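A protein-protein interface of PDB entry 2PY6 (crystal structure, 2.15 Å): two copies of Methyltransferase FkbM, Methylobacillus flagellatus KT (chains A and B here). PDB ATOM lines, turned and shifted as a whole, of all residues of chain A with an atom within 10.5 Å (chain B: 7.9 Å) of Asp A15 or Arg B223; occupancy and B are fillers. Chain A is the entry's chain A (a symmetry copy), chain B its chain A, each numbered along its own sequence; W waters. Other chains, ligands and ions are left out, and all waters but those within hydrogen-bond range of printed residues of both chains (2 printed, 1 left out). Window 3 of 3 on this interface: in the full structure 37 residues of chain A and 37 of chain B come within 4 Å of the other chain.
Among the printed residues, pairs that only touch across the chains: Asp A15 with Arg B223, Pro A16 with Gly B220, Pro A16 with Leu B221, Pro A16 with Leu B222, Leu A17 with Gly B220, Leu A17 with Leu B221, Leu A17 with Tyr B409, Glu A203 with Val B247 and Glu A207 with Ser B219.
NZ of Lys B364 sits close to O of Arg B223 (3.4 Å).
N of Leu B221 lies within hydrogen-bond range of OG of Ser B219 (3.1 Å).
The side-chain carboxylate (OE2) of Glu A201 lies within hydrogen-bond range of the backbone NH (N) of Glu A203.
The side-chain amide nitrogen (NE2) of Gln A188 lies within hydrogen-bond range of the backbone carbonyl oxygen (O) of Pro A16 (2.7 Å).
N of Leu A17 lies close to OD1 of Asp A15, at 3.2 Å.
Asp A15 touches one residue of chain B.
Of chain A, only Pro A16 comes within 4 Å of Leu B222.
No residue of chain A comes within 4 Å of Phe B224.
Of the printed residues of chain A, Tyr B409 touches Leu A17 (3.6 Å).
Of the printed residues of chain A, Leu B221 touches Pro A16 and Leu A17.
The nearest residue of chain B that does not touch Asp A15 is Leu B222 (5.4 Å).
The nearest residue of chain A that does not touch Arg B223 is Pro A16 (4.3 Å).
Of the 17 printed residues of chain B, 7 touch a printed residue of chain A.
Printed residues of chain B that touch a printed residue of chain A: Ser B219, Gly B220, Leu B221, Leu B222, Arg B223, Val B247 and Tyr B409.
Hydrophobic or aromatic side chains of chain B that line the printed part of chain A: Val B247 and Tyr B409.
Among the printed residues, 11 pairs touch across the chains.
Among the printed residues, no Asp or Glu carboxylate lies within 4 Å of a Lys or Arg side-chain nitrogen of the other chain.
No position is printed for both chains.
Of the 11 pairs that touch across the chains among the printed residues, none has its exchanged pair printed and touching as well.
Water W1 bridges the backbone carbonyl oxygen (O) of Leu B222 and the side-chain carboxylate (OE1) of Glu A207.
Water W2 bridges the backbone carbonyl oxygen (O) of Ser B219 (2.9 Å) and the backbone carbonyl oxygen (O) of Glu A207 (3.4 Å).
The side-chain carboxylate (OE1) of Glu A207 sits at hydrogen-bond distance from the backbone NH (N) of Gly B220, at 3.0 Å.
The backbone carbonyl oxygen of Gly B220 is in hydrogen-bond range of the side-chain amide nitrogen of Gln A188, 3.0 Å away.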
ATOM      1  N   ASP A  15      14.212 -30.694  13.887  1.00  0.00           N
ATOM      2  CA  ASP A  15      13.248 -29.531  13.867  1.00  0.00           C
ATOM      3  C   ASP A  15      13.922 -28.198  14.307  1.00  0.00           C
ATOM      4  O   ASP A  15      13.860 -27.807  15.496  1.00  0.00           O
ATOM      5  CB  ASP A  15      11.990 -29.805  14.710  1.00  0.00           C
ATOM      6  CG  ASP A  15      10.875 -28.753  14.479  1.00  0.00           C
ATOM      7  OD1 ASP A  15      11.029 -27.810  13.648  1.00  0.00           O
ATOM      8  OD2 ASP A  15       9.817 -28.879  15.132  1.00  0.00           O
ATOM      9  N   PRO A  16      14.449 -27.433  13.325  1.00  0.00           N
ATOM     10  CA  PRO A  16      15.215 -26.268  13.683  1.00  0.00           C
ATOM     11  C   PRO A  16      14.321 -25.141  14.154  1.00  0.00           C
ATOM     12  O   PRO A  16      14.824 -24.101  14.589  1.00  0.00           O
ATOM     13  CB  PRO A  16      15.934 -25.923  12.375  1.00  0.00           C
ATOM     14  CG  PRO A  16      14.992 -26.305  11.351  1.00  0.00           C
ATOM     15  CD  PRO A  16      14.286 -27.527  11.858  1.00  0.00           C
ATOM     16  N   LEU A  17      13.006 -25.331  14.071  1.00  0.00           N
ATOM     17  CA  LEU A  17      12.092 -24.324  14.533  1.00  0.00           C
ATOM     18  C   LEU A  17      11.728 -24.513  16.007  1.00  0.00           C
ATOM     19  O   LEU A  17      10.949 -23.697  16.526  1.00  0.00           O
ATOM     20  CB  LEU A  17      10.852 -24.255  13.631  1.00  0.00           C
ATOM     21  CG  LEU A  17      11.107 -23.592  12.274  1.00  0.00           C
ATOM     22  CD1 LEU A  17       9.843 -23.518  11.504  1.00  0.00           C
ATOM     23  CD2 LEU A  17      11.689 -22.189  12.383  1.00  0.00           C
ATOM     24  N   ALA A  18      12.326 -25.533  16.663  1.00  0.00           N
ATOM     25  CA  ALA A  18      12.084 -25.860  18.080  1.00  0.00           C
ATOM     26  C   ALA A  18      13.380 -26.297  18.794  1.00  0.00           C
ATOM     27  O   ALA A  18      13.413 -27.258  19.560  1.00  0.00           O
ATOM     28  CB  ALA A  18      11.036 -26.968  18.183  1.00  0.00           C
ATOM     29  N   MET A  19      14.459 -25.590  18.516  1.00  0.00           N
ATOM     30  CA  MET A  19      15.734 -25.901  19.124  1.00  0.00           C
ATOM     31  C   MET A  19      15.843 -25.620  20.601  1.00  0.00           C
ATOM     32  O   MET A  19      16.753 -26.138  21.262  1.00  0.00           O
ATOM     33  CB  MET A  19      16.868 -25.252  18.359  1.00  0.00           C
ATOM     34  CG  MET A  19      16.868 -25.734  16.916  1.00  0.00           C
ATOM     35  SD  MET A  19      18.599 -25.730  16.339  1.00  0.00           S
ATOM     36  CE  MET A  19      18.576 -25.698  14.526  1.00  0.00           C
ATOM     37  N   ASN A  20      14.932 -24.794  21.099  1.00  0.00           N
ATOM     38  CA  ASN A  20      14.795 -24.526  22.529  1.00  0.00           C
ATOM     39  C   ASN A  20      14.320 -25.817  23.207  1.00  0.00           C
ATOM     40  O   ASN A  20      14.864 -26.240  24.235  1.00  0.00           O
ATOM     41  CB  ASN A  20      13.832 -23.335  22.779  1.00  0.00           C
ATOM     42  CG  ASN A  20      12.429 -23.522  22.141  1.00  0.00           C
ATOM     43  OD1 ASN A  20      12.269 -24.055  21.023  1.00  0.00           O
ATOM     44  ND2 ASN A  20      11.417 -23.084  22.865  1.00  0.00           N
ATOM     45  N   ASP A  21      13.358 -26.488  22.584  1.00  0.00           N
ATOM     46  CA  ASP A  21      12.865 -27.734  23.123  1.00  0.00           C
ATOM     47  C   ASP A  21      13.913 -28.833  23.103  1.00  0.00           C
ATOM     48  O   ASP A  21      14.108 -29.522  24.114  1.00  0.00           O
ATOM     49  CB  ASP A  21      11.609 -28.170  22.383  1.00  0.00           C
ATOM     50  CG  ASP A  21      10.424 -27.262  22.677  1.00  0.00           C
ATOM     51  OD1 ASP A  21      10.405 -26.626  23.747  1.00  0.00           O
ATOM     52  OD2 ASP A  21       9.492 -27.223  21.862  1.00  0.00           O
ATOM     53  N   SER A  22      14.572 -29.007  21.964  1.00  0.00           N
ATOM     54  CA  SER A  22      15.611 -30.017  21.845  1.00  0.00           C
ATOM     55  C   SER A  22      16.768 -29.744  22.841  1.00  0.00           C
ATOM     56  O   SER A  22      17.403 -30.686  23.366  1.00  0.00           O
ATOM     57  CB  SER A  22      16.083 -30.143  20.376  1.00  0.00           C
ATOM     58  OG  SER A  22      16.652 -28.944  19.906  1.00  0.00           O
ATOM     59  N   PHE A  23      17.037 -28.463  23.108  1.00  0.00           N
ATOM     60  CA  PHE A  23      18.088 -28.057  24.059  1.00  0.00           C
ATOM     61  C   PHE A  23      17.843 -28.627  25.465  1.00  0.00           C
ATOM     62  O   PHE A  23      18.748 -29.227  26.075  1.00  0.00           O
ATOM     63  CB  PHE A  23      18.229 -26.506  24.094  1.00  0.00           C
ATOM     64  CG  PHE A  23      18.968 -25.953  25.307  1.00  0.00           C
ATOM     65  CD1 PHE A  23      20.341 -26.130  25.457  1.00  0.00           C
ATOM     66  CD2 PHE A  23      18.287 -25.215  26.275  1.00  0.00           C
ATOM     67  CE1 PHE A  23      21.026 -25.599  26.542  1.00  0.00           C
ATOM     68  CE2 PHE A  23      18.964 -24.665  27.353  1.00  0.00           C
ATOM     69  CZ  PHE A  23      20.342 -24.850  27.489  1.00  0.00           C
ATOM     70  N   GLN A 188      17.974 -18.717  17.744  1.00  0.00           N
ATOM     71  CA  GLN A 188      18.144 -20.009  17.079  1.00  0.00           C
ATOM     72  C   GLN A 188      19.637 -20.413  17.055  1.00  0.00           C
ATOM     73  O   GLN A 188      20.005 -21.576  17.307  1.00  0.00           O
ATOM     74  CB  GLN A 188      17.558 -19.983  15.677  1.00  0.00           C
ATOM     75  CG  GLN A 188      17.287 -21.412  15.106  1.00  0.00           C
ATOM     76  CD  GLN A 188      17.032 -21.392  13.613  1.00  0.00           C
ATOM     77  OE1 GLN A 188      17.562 -20.530  12.877  1.00  0.00           O
ATOM     78  NE2 GLN A 188      16.211 -22.332  13.147  1.00  0.00           N
ATOM     79  N   TYR A 191      20.831 -21.640  20.605  1.00  0.00           N
ATOM     80  CA  TYR A 191      20.380 -22.997  20.864  1.00  0.00           C
ATOM     81  C   TYR A 191      21.040 -24.050  19.980  1.00  0.00           C
ATOM     82  O   TYR A 191      21.357 -25.133  20.461  1.00  0.00           O
ATOM     83  CB  TYR A 191      18.869 -23.102  20.829  1.00  0.00           C
ATOM     84  CG  TYR A 191      18.176 -22.447  22.025  1.00  0.00           C
ATOM     85  CD1 TYR A 191      18.480 -22.814  23.328  1.00  0.00           C
ATOM     86  CD2 TYR A 191      17.179 -21.510  21.838  1.00  0.00           C
ATOM     87  CE1 TYR A 191      17.843 -22.228  24.409  1.00  0.00           C
ATOM     88  CE2 TYR A 191      16.541 -20.921  22.906  1.00  0.00           C
ATOM     89  CZ  TYR A 191      16.860 -21.283  24.187  1.00  0.00           C
ATOM     90  OH  TYR A 191      16.202 -20.695  25.259  1.00  0.00           O
ATOM     91  N   ALA A 192      21.342 -23.698  18.728  1.00  0.00           N
ATOM     92  CA  ALA A 192      22.034 -24.603  17.794  1.00  0.00           C
ATOM     93  C   ALA A 192      23.465 -24.916  18.300  1.00  0.00           C
ATOM     94  O   ALA A 192      23.905 -26.066  18.324  1.00  0.00           O
ATOM     95  CB  ALA A 192      22.044 -23.989  16.380  1.00  0.00           C
ATOM     96  N   ASN A 195      23.160 -27.052  21.437  1.00  0.00           N
ATOM     97  CA  ASN A 195      22.749 -28.392  21.031  1.00  0.00           C
ATOM     98  C   ASN A 195      23.917 -29.163  20.421  1.00  0.00           C
ATOM     99  O   ASN A 195      24.061 -30.341  20.710  1.00  0.00           O
ATOM    100  CB  ASN A 195      21.535 -28.373  20.118  1.00  0.00           C
ATOM    101  CG  ASN A 195      20.270 -27.975  20.856  1.00  0.00           C
ATOM    102  OD1 ASN A 195      20.246 -27.987  22.065  1.00  0.00           O
ATOM    103  ND2 ASN A 195      19.248 -27.574  20.132  1.00  0.00           N
ATOM    104  N   GLU A 201      26.453 -33.427  17.572  1.00  0.00           N
ATOM    105  CA  GLU A 201      25.904 -33.471  16.230  1.00  0.00           C
ATOM    106  C   GLU A 201      26.180 -32.175  15.473  1.00  0.00           C
ATOM    107  O   GLU A 201      25.506 -31.174  15.694  1.00  0.00           O
ATOM    108  CB  GLU A 201      24.373 -33.733  16.271  1.00  0.00           C
ATOM    109  CG  GLU A 201      23.681 -33.647  14.893  1.00  0.00           C
ATOM    110  CD  GLU A 201      24.349 -34.503  13.799  1.00  0.00           C
ATOM    111  OE1 GLU A 201      24.242 -35.730  13.838  1.00  0.00           O
ATOM    112  OE2 GLU A 201      24.951 -33.939  12.866  1.00  0.00           O
ATOM    113  N   GLU A 203      25.428 -31.122  12.529  1.00  0.00           N
ATOM    114  CA  GLU A 203      24.317 -30.578  11.741  1.00  0.00           C
ATOM    115  C   GLU A 203      23.631 -29.405  12.463  1.00  0.00           C
ATOM    116  O   GLU A 203      22.998 -28.576  11.800  1.00  0.00           O
ATOM    117  CB  GLU A 203      23.297 -31.656  11.353  1.00  0.00           C
ATOM    118  CG  GLU A 203      23.767 -32.664  10.296  1.00  0.00           C
ATOM    119  CD  GLU A 203      24.118 -32.022   8.943  1.00  0.00           C
ATOM    120  OE1 GLU A 203      23.398 -31.116   8.462  1.00  0.00           O
ATOM    121  OE2 GLU A 203      25.115 -32.446   8.345  1.00  0.00           O
ATOM    122  N   TYR A 204      23.741 -29.332  13.796  1.00  0.00           N
ATOM    123  CA  TYR A 204      23.195 -28.170  14.520  1.00  0.00           C
ATOM    124  C   TYR A 204      23.819 -26.839  14.060  1.00  0.00           C
ATOM    125  O   TYR A 204      23.077 -25.889  13.834  1.00  0.00           O
ATOM    126  CB  TYR A 204      23.273 -28.334  16.038  1.00  0.00           C
ATOM    127  CG  TYR A 204      22.173 -29.181  16.557  1.00  0.00           C
ATOM    128  CD1 TYR A 204      20.892 -28.671  16.651  1.00  0.00           C
ATOM    129  CD2 TYR A 204      22.399 -30.501  16.954  1.00  0.00           C
ATOM    130  CE1 TYR A 204      19.849 -29.482  17.071  1.00  0.00           C
ATOM    131  CE2 TYR A 204      21.369 -31.313  17.410  1.00  0.00           C
ATOM    132  CZ  TYR A 204      20.101 -30.794  17.478  1.00  0.00           C
ATOM    133  OH  TYR A 204      19.067 -31.576  17.926  1.00  0.00           O
ATOM    134  N   GLU A 207      22.610 -25.710  10.411  1.00  0.00           N
ATOM    135  CA  GLU A 207      21.294 -25.102  10.261  1.00  0.00           C
ATOM    136  C   GLU A 207      21.332 -23.591  10.378  1.00  0.00           C
ATOM    137  O   GLU A 207      20.469 -22.908   9.848  1.00  0.00           O
ATOM    138  CB  GLU A 207      20.314 -25.620  11.353  1.00  0.00           C
ATOM    139  CG  GLU A 207      19.887 -27.050  11.249  1.00  0.00           C
ATOM    140  CD  GLU A 207      18.931 -27.395  10.107  1.00  0.00           C
ATOM    141  OE1 GLU A 207      18.519 -26.561   9.264  1.00  0.00           O
ATOM    142  OE2 GLU A 207      18.611 -28.577  10.045  1.00  0.00           O
ATOM    143  N   VAL A 208      22.318 -23.069  11.087  1.00  0.00           N
ATOM    144  CA  VAL A 208      22.398 -21.629  11.346  1.00  0.00           C
ATOM    145  C   VAL A 208      23.642 -20.893  10.793  1.00  0.00           C
ATOM    146  O   VAL A 208      23.651 -19.682  10.728  1.00  0.00           O
ATOM    147  CB  VAL A 208      22.336 -21.356  12.882  1.00  0.00           C
ATOM    148  CG1 VAL A 208      21.029 -21.879  13.468  1.00  0.00           C
ATOM    149  CG2 VAL A 208      23.560 -21.962  13.635  1.00  0.00           C
ATOM    150  N   TYR B 216      18.701 -26.001   0.646  1.00  0.00           N
ATOM    151  CA  TYR B 216      17.595 -26.973   0.730  1.00  0.00           C
ATOM    152  C   TYR B 216      17.486 -27.769   2.003  1.00  0.00           C
ATOM    153  O   TYR B 216      16.391 -27.911   2.518  1.00  0.00           O
ATOM    154  CB  TYR B 216      17.580 -27.996  -0.436  1.00  0.00           C
ATOM    155  CG  TYR B 216      17.771 -27.415  -1.811  1.00  0.00           C
ATOM    156  CD1 TYR B 216      16.946 -26.392  -2.293  1.00  0.00           C
ATOM    157  CD2 TYR B 216      18.727 -27.934  -2.666  1.00  0.00           C
ATOM    158  CE1 TYR B 216      17.114 -25.882  -3.585  1.00  0.00           C
ATOM    159  CE2 TYR B 216      18.917 -27.403  -3.946  1.00  0.00           C
ATOM    160  CZ  TYR B 216      18.119 -26.393  -4.401  1.00  0.00           C
ATOM    161  OH  TYR B 216      18.340 -25.884  -5.678  1.00  0.00           O
ATOM    162  N   PHE B 217      18.623 -28.321   2.465  1.00  0.00           N
ATOM    163  CA  PHE B 217      18.665 -29.284   3.555  1.00  0.00           C
ATOM    164  C   PHE B 217      19.062 -28.732   4.911  1.00  0.00           C
ATOM    165  O   PHE B 217      18.735 -29.358   5.919  1.00  0.00           O
ATOM    166  CB  PHE B 217      19.582 -30.442   3.148  1.00  0.00           C
ATOM    167  CG  PHE B 217      19.114 -31.154   1.896  1.00  0.00           C
ATOM    168  CD1 PHE B 217      17.977 -31.963   1.927  1.00  0.00           C
ATOM    169  CD2 PHE B 217      19.761 -30.965   0.689  1.00  0.00           C
ATOM    170  CE1 PHE B 217      17.491 -32.588   0.770  1.00  0.00           C
ATOM    171  CE2 PHE B 217      19.296 -31.583  -0.475  1.00  0.00           C
ATOM    172  CZ  PHE B 217      18.156 -32.406  -0.426  1.00  0.00           C
ATOM    173  N   SER B 219      18.536 -25.168   5.784  1.00  0.00           N
ATOM    174  CA  SER B 219      18.036 -23.782   5.748  1.00  0.00           C
ATOM    175  C   SER B 219      17.685 -23.139   7.088  1.00  0.00           C
ATOM    176  O   SER B 219      17.513 -21.917   7.162  1.00  0.00           O
ATOM    177  CB  SER B 219      16.774 -23.690   4.882  1.00  0.00           C
ATOM    178  OG  SER B 219      15.643 -24.287   5.503  1.00  0.00           O
ATOM    179  N   GLY B 220      17.557 -23.956   8.134  1.00  0.00           N
ATOM    180  CA  GLY B 220      17.081 -23.492   9.413  1.00  0.00           C
ATOM    181  C   GLY B 220      15.547 -23.473   9.496  1.00  0.00           C
ATOM    182  O   GLY B 220      14.995 -23.005  10.478  1.00  0.00           O
ATOM    183  N   LEU B 221      14.855 -24.005   8.495  1.00  0.00           N
ATOM    184  CA  LEU B 221      13.388 -23.922   8.447  1.00  0.00           C
ATOM    185  C   LEU B 221      12.635 -25.227   8.323  1.00  0.00           C
ATOM    186  O   LEU B 221      11.483 -25.301   8.777  1.00  0.00           O
ATOM    187  CB  LEU B 221      12.956 -22.997   7.268  1.00  0.00           C
ATOM    188  CG  LEU B 221      13.320 -21.522   7.369  1.00  0.00           C
ATOM    189  CD1 LEU B 221      13.109 -20.810   6.035  1.00  0.00           C
ATOM    190  CD2 LEU B 221      12.593 -20.845   8.495  1.00  0.00           C
ATOM    191  N   LEU B 222      13.268 -26.233   7.713  1.00  0.00           N
ATOM    192  CA  LEU B 222      12.661 -27.548   7.455  1.00  0.00           C
ATOM    193  C   LEU B 222      13.154 -28.702   8.321  1.00  0.00           C
ATOM    194  O   LEU B 222      14.312 -28.788   8.655  1.00  0.00           O
ATOM    195  CB  LEU B 222      12.896 -27.944   6.001  1.00  0.00           C
ATOM    196  CG  LEU B 222      12.403 -26.975   4.908  1.00  0.00           C
ATOM    197  CD1 LEU B 222      12.710 -27.593   3.594  1.00  0.00           C
ATOM    198  CD2 LEU B 222      10.910 -26.625   4.986  1.00  0.00           C
ATOM    199  N   ARG B 223      12.235 -29.600   8.650  1.00  0.00           N
ATOM    200  CA  ARG B 223      12.521 -30.817   9.381  1.00  0.00           C
ATOM    201  C   ARG B 223      12.395 -31.997   8.395  1.00  0.00           C
ATOM    202  O   ARG B 223      11.364 -32.155   7.742  1.00  0.00           O
ATOM    203  CB  ARG B 223      11.473 -31.011  10.479  1.00  0.00           C
ATOM    204  CG  ARG B 223      11.852 -32.008  11.539  1.00  0.00           C
ATOM    205  CD  ARG B 223      10.630 -32.473  12.350  1.00  0.00           C
ATOM    206  NE  ARG B 223      10.029 -33.683  11.762  1.00  0.00           N
ATOM    207  CZ  ARG B 223      10.510 -34.927  11.927  1.00  0.00           C
ATOM    208  NH1 ARG B 223      11.612 -35.156  12.636  1.00  0.00           N
ATOM    209  NH2 ARG B 223       9.893 -35.969  11.379  1.00  0.00           N
ATOM    210  N   PHE B 224      13.414 -32.835   8.327  1.00  0.00           N
ATOM    211  CA  PHE B 224      13.374 -34.001   7.500  1.00  0.00           C
ATOM    212  C   PHE B 224      13.274 -35.218   8.432  1.00  0.00           C
ATOM    213  O   PHE B 224      13.959 -35.291   9.450  1.00  0.00           O
ATOM    214  CB  PHE B 224      14.610 -34.081   6.612  1.00  0.00           C
ATOM    215  CG  PHE B 224      14.749 -32.920   5.678  1.00  0.00           C
ATOM    216  CD1 PHE B 224      14.104 -32.913   4.451  1.00  0.00           C
ATOM    217  CD2 PHE B 224      15.487 -31.816   6.039  1.00  0.00           C
ATOM    218  CE1 PHE B 224      14.193 -31.831   3.605  1.00  0.00           C
ATOM    219  CE2 PHE B 224      15.588 -30.725   5.196  1.00  0.00           C
ATOM    220  CZ  PHE B 224      14.937 -30.733   3.969  1.00  0.00           C
ATOM    221  N   SER B 225      12.415 -36.173   8.072  1.00  0.00           N
ATOM    222  CA  SER B 225      12.253 -37.376   8.831  1.00  0.00           C
ATOM    223  C   SER B 225      13.168 -38.433   8.219  1.00  0.00           C
ATOM    224  O   SER B 225      13.964 -38.159   7.317  1.00  0.00           O
ATOM    225  CB  SER B 225      10.811 -37.836   8.734  1.00  0.00           C
ATOM    226  OG  SER B 225      10.587 -38.300   7.428  1.00  0.00           O
ATOM    227  N   ASP B 226      13.040 -39.651   8.708  1.00  0.00           N
ATOM    228  CA  ASP B 226      13.777 -40.788   8.150  1.00  0.00           C
ATOM    229  C   ASP B 226      13.016 -41.551   7.023  1.00  0.00           C
ATOM    230  O   ASP B 226      13.480 -42.590   6.553  1.00  0.00           O
ATOM    231  CB  ASP B 226      14.168 -41.736   9.299  1.00  0.00           C
ATOM    232  CG  ASP B 226      12.964 -42.404   9.972  1.00  0.00           C
ATOM    233  OD1 ASP B 226      11.791 -42.001   9.720  1.00  0.00           O
ATOM    234  OD2 ASP B 226      13.208 -43.336  10.781  1.00  0.00           O
ATOM    235  N   SER B 227      11.874 -41.012   6.577  1.00  0.00           N
ATOM    236  CA  SER B 227      11.033 -41.668   5.584  1.00  0.00           C
ATOM    237  C   SER B 227      10.627 -40.688   4.488  1.00  0.00           C
ATOM    238  O   SER B 227       9.505 -40.741   3.954  1.00  0.00           O
ATOM    239  CB  SER B 227       9.760 -42.149   6.262  1.00  0.00           C
ATOM    240  OG  SER B 227      10.074 -42.830   7.443  1.00  0.00           O
ATOM    241  N   GLU B 228      11.538 -39.802   4.128  1.00  0.00           N
ATOM    242  CA  GLU B 228      11.210 -38.793   3.139  1.00  0.00           C
ATOM    243  C   GLU B 228      11.042 -39.419   1.756  1.00  0.00           C
ATOM    244  O   GLU B 228      11.674 -40.413   1.450  1.00  0.00           O
ATOM    245  CB  GLU B 228      12.289 -37.717   3.111  1.00  0.00           C
ATOM    246  CG  GLU B 228      12.382 -36.908   4.432  1.00  0.00           C
ATOM    247  CD  GLU B 228      11.367 -35.790   4.539  1.00  0.00           C
ATOM    248  OE1 GLU B 228      10.848 -35.331   3.500  1.00  0.00           O
ATOM    249  OE2 GLU B 228      11.119 -35.307   5.667  1.00  0.00           O
ATOM    250  N   VAL B 247      21.898 -35.512   5.406  1.00  0.00           N
ATOM    251  CA  VAL B 247      21.108 -35.020   6.555  1.00  0.00           C
ATOM    252  C   VAL B 247      20.214 -36.066   7.167  1.00  0.00           C
ATOM    253  O   VAL B 247      19.866 -35.941   8.320  1.00  0.00           O
ATOM    254  CB  VAL B 247      20.288 -33.737   6.265  1.00  0.00           C
ATOM    255  CG1 VAL B 247      21.227 -32.649   5.814  1.00  0.00           C
ATOM    256  CG2 VAL B 247      19.155 -33.994   5.247  1.00  0.00           C
ATOM    257  N   THR B 337       6.827 -36.088   0.176  1.00  0.00           N
ATOM    258  CA  THR B 337       6.967 -35.358   1.420  1.00  0.00           C
ATOM    259  C   THR B 337       7.821 -34.098   1.209  1.00  0.00           C
ATOM    260  O   THR B 337       7.806 -33.219   2.052  1.00  0.00           O
ATOM    261  CB  THR B 337       7.657 -36.256   2.494  1.00  0.00           C
ATOM    262  OG1 THR B 337       8.978 -36.620   2.063  1.00  0.00           O
ATOM    263  CG2 THR B 337       6.842 -37.542   2.761  1.00  0.00           C
ATOM    264  N   PHE B 338       8.532 -34.012   0.077  1.00  0.00           N
ATOM    265  CA  PHE B 338       9.428 -32.907  -0.217  1.00  0.00           C
ATOM    266  C   PHE B 338       9.617 -32.737  -1.712  1.00  0.00           C
ATOM    267  O   PHE B 338       9.852 -33.716  -2.431  1.00  0.00           O
ATOM    268  CB  PHE B 338      10.788 -33.189   0.459  1.00  0.00           C
ATOM    269  CG  PHE B 338      11.824 -32.121   0.261  1.00  0.00           C
ATOM    270  CD1 PHE B 338      11.535 -30.777   0.527  1.00  0.00           C
ATOM    271  CD2 PHE B 338      13.120 -32.457  -0.076  1.00  0.00           C
ATOM    272  CE1 PHE B 338      12.472 -29.801   0.375  1.00  0.00           C
ATOM    273  CE2 PHE B 338      14.085 -31.471  -0.235  1.00  0.00           C
ATOM    274  CZ  PHE B 338      13.766 -30.138  -0.007  1.00  0.00           C
ATOM    275  N   LYS B 364       6.744 -30.445   1.948  1.00  0.00           N
ATOM    276  CA  LYS B 364       7.678 -29.358   2.120  1.00  0.00           C
ATOM    277  C   LYS B 364       8.169 -29.013   0.724  1.00  0.00           C
ATOM    278  O   LYS B 364       8.237 -29.889  -0.157  1.00  0.00           O
ATOM    279  CB  LYS B 364       8.872 -29.778   2.982  1.00  0.00           C
ATOM    280  CG  LYS B 364       8.584 -30.145   4.401  1.00  0.00           C
ATOM    281  CD  LYS B 364       9.853 -30.580   5.167  1.00  0.00           C
ATOM    282  CE  LYS B 364      10.465 -31.885   4.696  1.00  0.00           C
ATOM    283  NZ  LYS B 364       9.587 -32.998   5.010  1.00  0.00           N
ATOM    284  N   TYR B 409       6.489 -24.758   4.085  1.00  0.00           N
ATOM    285  CA  TYR B 409       6.332 -25.865   4.997  1.00  0.00           C
ATOM    286  C   TYR B 409       5.100 -25.658   5.857  1.00  0.00           C
ATOM    287  O   TYR B 409       4.263 -24.741   5.652  1.00  0.00           O
ATOM    288  CB  TYR B 409       7.606 -25.957   5.880  1.00  0.00           C
ATOM    289  CG  TYR B 409       7.878 -24.679   6.635  1.00  0.00           C
ATOM    290  CD1 TYR B 409       8.607 -23.635   6.055  1.00  0.00           C
ATOM    291  CD2 TYR B 409       7.410 -24.496   7.917  1.00  0.00           C
ATOM    292  CE1 TYR B 409       8.830 -22.458   6.735  1.00  0.00           C
ATOM    293  CE2 TYR B 409       7.655 -23.300   8.616  1.00  0.00           C
ATOM    294  CZ  TYR B 409       8.364 -22.307   8.021  1.00  0.00           C
ATOM    295  OH  TYR B 409       8.600 -21.146   8.712  1.00  0.00           O
ATOM    296  OXT TYR B 409       4.988 -26.403   6.837  1.00  0.00           O
HETATM  297  O   HOH W   1      16.253 -27.381   7.632  1.00  0.00           O
HETATM  298  O   HOH W   2      19.151 -20.009   8.622  1.00  0.00           O
